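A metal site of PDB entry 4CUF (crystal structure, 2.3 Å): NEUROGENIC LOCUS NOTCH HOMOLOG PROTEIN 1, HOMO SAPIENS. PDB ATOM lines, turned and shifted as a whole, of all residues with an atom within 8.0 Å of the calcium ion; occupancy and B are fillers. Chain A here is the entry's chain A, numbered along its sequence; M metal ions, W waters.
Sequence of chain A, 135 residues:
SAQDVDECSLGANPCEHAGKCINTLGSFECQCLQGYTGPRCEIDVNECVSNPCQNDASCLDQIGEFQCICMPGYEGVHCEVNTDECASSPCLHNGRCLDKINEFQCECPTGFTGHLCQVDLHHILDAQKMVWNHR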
ATOM      1  N   ASP A   4      25.418  20.879  13.805  1.00  0.00           N
ATOM      2  CA  ASP A   4      24.442  21.545  14.672  1.00  0.00           C
ATOM      3  C   ASP A   4      23.140  21.908  13.921  1.00  0.00           C
ATOM      4  O   ASP A   4      22.341  21.003  13.643  1.00  0.00           O
ATOM      5  CB  ASP A   4      25.047  22.753  15.462  1.00  0.00           C
ATOM      6  CG  ASP A   4      24.807  22.756  16.986  1.00  0.00           C
ATOM      7  OD1 ASP A   4      23.920  22.010  17.460  1.00  0.00           O
ATOM      8  OD2 ASP A   4      25.486  23.519  17.694  1.00  0.00           O
ATOM      9  N   VAL A   5      22.948  23.214  13.578  1.00  0.00           N
ATOM     10  CA  VAL A   5      21.767  23.889  13.005  1.00  0.00           C
ATOM     11  C   VAL A   5      22.217  24.887  11.932  1.00  0.00           C
ATOM     12  O   VAL A   5      23.289  25.476  12.076  1.00  0.00           O
ATOM     13  CB  VAL A   5      21.113  24.751  14.141  1.00  0.00           C
ATOM     14  CG1 VAL A   5      19.872  25.499  13.697  1.00  0.00           C
ATOM     15  CG2 VAL A   5      20.856  23.990  15.413  1.00  0.00           C
ATOM     16  N   ASP A   6      21.376  25.139  10.926  1.00  0.00           N
ATOM     17  CA  ASP A   6      21.584  26.207   9.975  1.00  0.00           C
ATOM     18  C   ASP A   6      20.808  27.409  10.501  1.00  0.00           C
ATOM     19  O   ASP A   6      19.613  27.542  10.225  1.00  0.00           O
ATOM     20  CB  ASP A   6      21.094  25.846   8.569  1.00  0.00           C
ATOM     21  CG  ASP A   6      21.337  26.942   7.539  1.00  0.00           C
ATOM     22  OD1 ASP A   6      21.723  28.092   7.948  1.00  0.00           O
ATOM     23  OD2 ASP A   6      21.142  26.680   6.338  1.00  0.00           O
ATOM     24  N   GLU A   7      21.479  28.297  11.235  1.00  0.00           N
ATOM     25  CA  GLU A   7      20.872  29.516  11.809  1.00  0.00           C
ATOM     26  C   GLU A   7      20.322  30.472  10.743  1.00  0.00           C
ATOM     27  O   GLU A   7      19.448  31.277  11.070  1.00  0.00           O
ATOM     28  CB  GLU A   7      21.880  30.274  12.680  1.00  0.00           C
ATOM     29  CG  GLU A   7      22.256  29.505  13.945  1.00  0.00           C
ATOM     30  CD  GLU A   7      23.476  28.611  13.821  1.00  0.00           C
ATOM     31  OE1 GLU A   7      23.884  28.268  12.688  1.00  0.00           O
ATOM     32  OE2 GLU A   7      24.035  28.237  14.879  1.00  0.00           O
ATOM     33  N   CYS A   8      20.813  30.369   9.486  1.00  0.00           N
ATOM     34  CA  CYS A   8      20.388  31.210   8.360  1.00  0.00           C
ATOM     35  C   CYS A   8      19.053  30.727   7.777  1.00  0.00           C
ATOM     36  O   CYS A   8      18.507  31.432   6.928  1.00  0.00           O
ATOM     37  CB  CYS A   8      21.475  31.283   7.290  1.00  0.00           C
ATOM     38  SG  CYS A   8      23.114  31.746   7.909  1.00  0.00           S
ATOM     39  N   ILE A  22      25.750  33.610   6.571  1.00  0.00           N
ATOM     40  CA  ILE A  22      26.500  32.459   6.041  1.00  0.00           C
ATOM     41  C   ILE A  22      26.560  31.368   7.124  1.00  0.00           C
ATOM     42  O   ILE A  22      27.059  31.610   8.229  1.00  0.00           O
ATOM     43  CB  ILE A  22      27.882  32.895   5.526  1.00  0.00           C
ATOM     44  CG1 ILE A  22      27.740  33.845   4.279  1.00  0.00           C
ATOM     45  CG2 ILE A  22      28.771  31.689   5.251  1.00  0.00           C
ATOM     46  CD1 ILE A  22      28.873  34.793   4.022  1.00  0.00           C
ATOM     47  N   ASN A  23      26.075  30.183   6.814  1.00  0.00           N
ATOM     48  CA  ASN A  23      26.094  29.146   7.823  1.00  0.00           C
ATOM     49  C   ASN A  23      27.476  28.504   7.981  1.00  0.00           C
ATOM     50  O   ASN A  23      28.189  28.332   7.000  1.00  0.00           O
ATOM     51  CB  ASN A  23      25.021  28.095   7.538  1.00  0.00           C
ATOM     52  CG  ASN A  23      24.883  27.047   8.609  1.00  0.00           C
ATOM     53  OD1 ASN A  23      24.890  27.349   9.808  1.00  0.00           O
ATOM     54  ND2 ASN A  23      24.734  25.785   8.196  1.00  0.00           N
ATOM     55  N   THR A  24      27.843  28.173   9.230  1.00  0.00           N
ATOM     56  CA  THR A  24      29.039  27.386   9.551  1.00  0.00           C
ATOM     57  C   THR A  24      28.634  26.215  10.459  1.00  0.00           C
ATOM     58  O   THR A  24      27.578  26.269  11.091  1.00  0.00           O
ATOM     59  CB  THR A  24      30.164  28.194  10.198  1.00  0.00           C
ATOM     60  OG1 THR A  24      29.889  28.470  11.568  1.00  0.00           O
ATOM     61  CG2 THR A  24      30.494  29.450   9.451  1.00  0.00           C
ATOM     62  N   LEU A  25      29.477  25.188  10.572  1.00  0.00           N
ATOM     63  CA  LEU A  25      29.189  24.109  11.494  1.00  0.00           C
ATOM     64  C   LEU A  25      29.536  24.581  12.902  1.00  0.00           C
ATOM     65  O   LEU A  25      30.687  24.933  13.180  1.00  0.00           O
ATOM     66  CB  LEU A  25      29.927  22.828  11.115  1.00  0.00           C
ATOM     67  CG  LEU A  25      29.504  22.142   9.805  1.00  0.00           C
ATOM     68  CD1 LEU A  25      30.447  21.015   9.472  1.00  0.00           C
ATOM     69  CD2 LEU A  25      28.072  21.571   9.877  1.00  0.00           C
ATOM     70  N   GLY A  26      28.516  24.659  13.740  1.00  0.00           N
ATOM     71  CA  GLY A  26      28.669  25.095  15.127  1.00  0.00           C
ATOM     72  C   GLY A  26      28.328  26.550  15.352  1.00  0.00           C
ATOM     73  O   GLY A  26      28.199  26.994  16.498  1.00  0.00           O
ATOM     74  N   SER A  27      28.189  27.316  14.281  1.00  0.00           N
ATOM     75  CA  SER A  27      27.823  28.725  14.383  1.00  0.00           C
ATOM     76  C   SER A  27      27.322  29.243  13.035  1.00  0.00           C
ATOM     77  O   SER A  27      26.790  28.498  12.224  1.00  0.00           O
ATOM     78  CB  SER A  27      28.990  29.563  14.909  1.00  0.00           C
ATOM     79  OG  SER A  27      28.524  30.801  15.433  1.00  0.00           O
ATOM     80  N   PHE A  28      27.498  30.513  12.813  1.00  0.00           N
ATOM     81  CA  PHE A  28      27.193  31.208  11.570  1.00  0.00           C
ATOM     82  C   PHE A  28      28.019  32.469  11.553  1.00  0.00           C
ATOM     83  O   PHE A  28      28.600  32.849  12.569  1.00  0.00           O
ATOM     84  CB  PHE A  28      25.679  31.523  11.431  1.00  0.00           C
ATOM     85  CG  PHE A  28      25.157  32.521  12.431  1.00  0.00           C
ATOM     86  CD1 PHE A  28      24.777  32.110  13.702  1.00  0.00           C
ATOM     87  CD2 PHE A  28      25.049  33.854  12.094  1.00  0.00           C
ATOM     88  CE1 PHE A  28      24.298  33.037  14.624  1.00  0.00           C
ATOM     89  CE2 PHE A  28      24.590  34.776  13.024  1.00  0.00           C
ATOM     90  CZ  PHE A  28      24.204  34.353  14.277  1.00  0.00           C
ATOM     91  N   GLU A  29      28.095  33.108  10.401  1.00  0.00           N
ATOM     92  CA  GLU A  29      28.793  34.368  10.259  1.00  0.00           C
ATOM     93  C   GLU A  29      27.967  35.331   9.440  1.00  0.00           C
ATOM     94  O   GLU A  29      27.097  34.894   8.651  1.00  0.00           O
ATOM     95  CB  GLU A  29      30.222  34.208   9.716  1.00  0.00           C
ATOM     96  CG  GLU A  29      30.299  33.577   8.327  1.00  0.00           C
ATOM     97  CD  GLU A  29      31.652  33.046   7.904  1.00  0.00           C
ATOM     98  OE1 GLU A  29      32.573  32.998   8.761  1.00  0.00           O
ATOM     99  OE2 GLU A  29      31.802  32.674   6.725  1.00  0.00           O
HETATM  100 CA    CA M   1      25.421  26.606  12.128  1.00  0.00          CA
HETATM  101  O   HOH W   1      25.079  23.778  11.114  1.00  0.00           O
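OG1 of Thr 24 sits close to N of Ser 27 (3.4 Å). OG1 of Thr 24 is in hydrogen-bond range of N of Phe 28 (3.4 Å). N of Asn 23 lies within hydrogen-bond range of SG of Cys 8, at 3.5 Å.
Residues that only touch the calcium ion: Gly 26 (3.996 Å). Within 4 Å of the calcium ion: Val 5, Glu 7, Asn 23, Thr 24, Gly 26 and Ser 27. The nearest printed residue that does not touch the calcium ion is Asp 6 (4.4 Å).
The calcium ion is bound by the side-chain carboxylate (OE1) of Glu 7 (2.3 Å), the backbone carbonyl oxygen (O) of Ser 27 (2.3 Å), the backbone carbonyl oxygen (O) of Val 5 (2.4 Å), the backbone carbonyl oxygen (O) of Thr 24 (2.4 Å) and the side-chain amide oxygen (OD1) of Asn 23 (2.5 Å). The calcium ion has five donor atoms within binding distance. Slightly farther from the calcium ion lies water W1 (3.0 Å).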
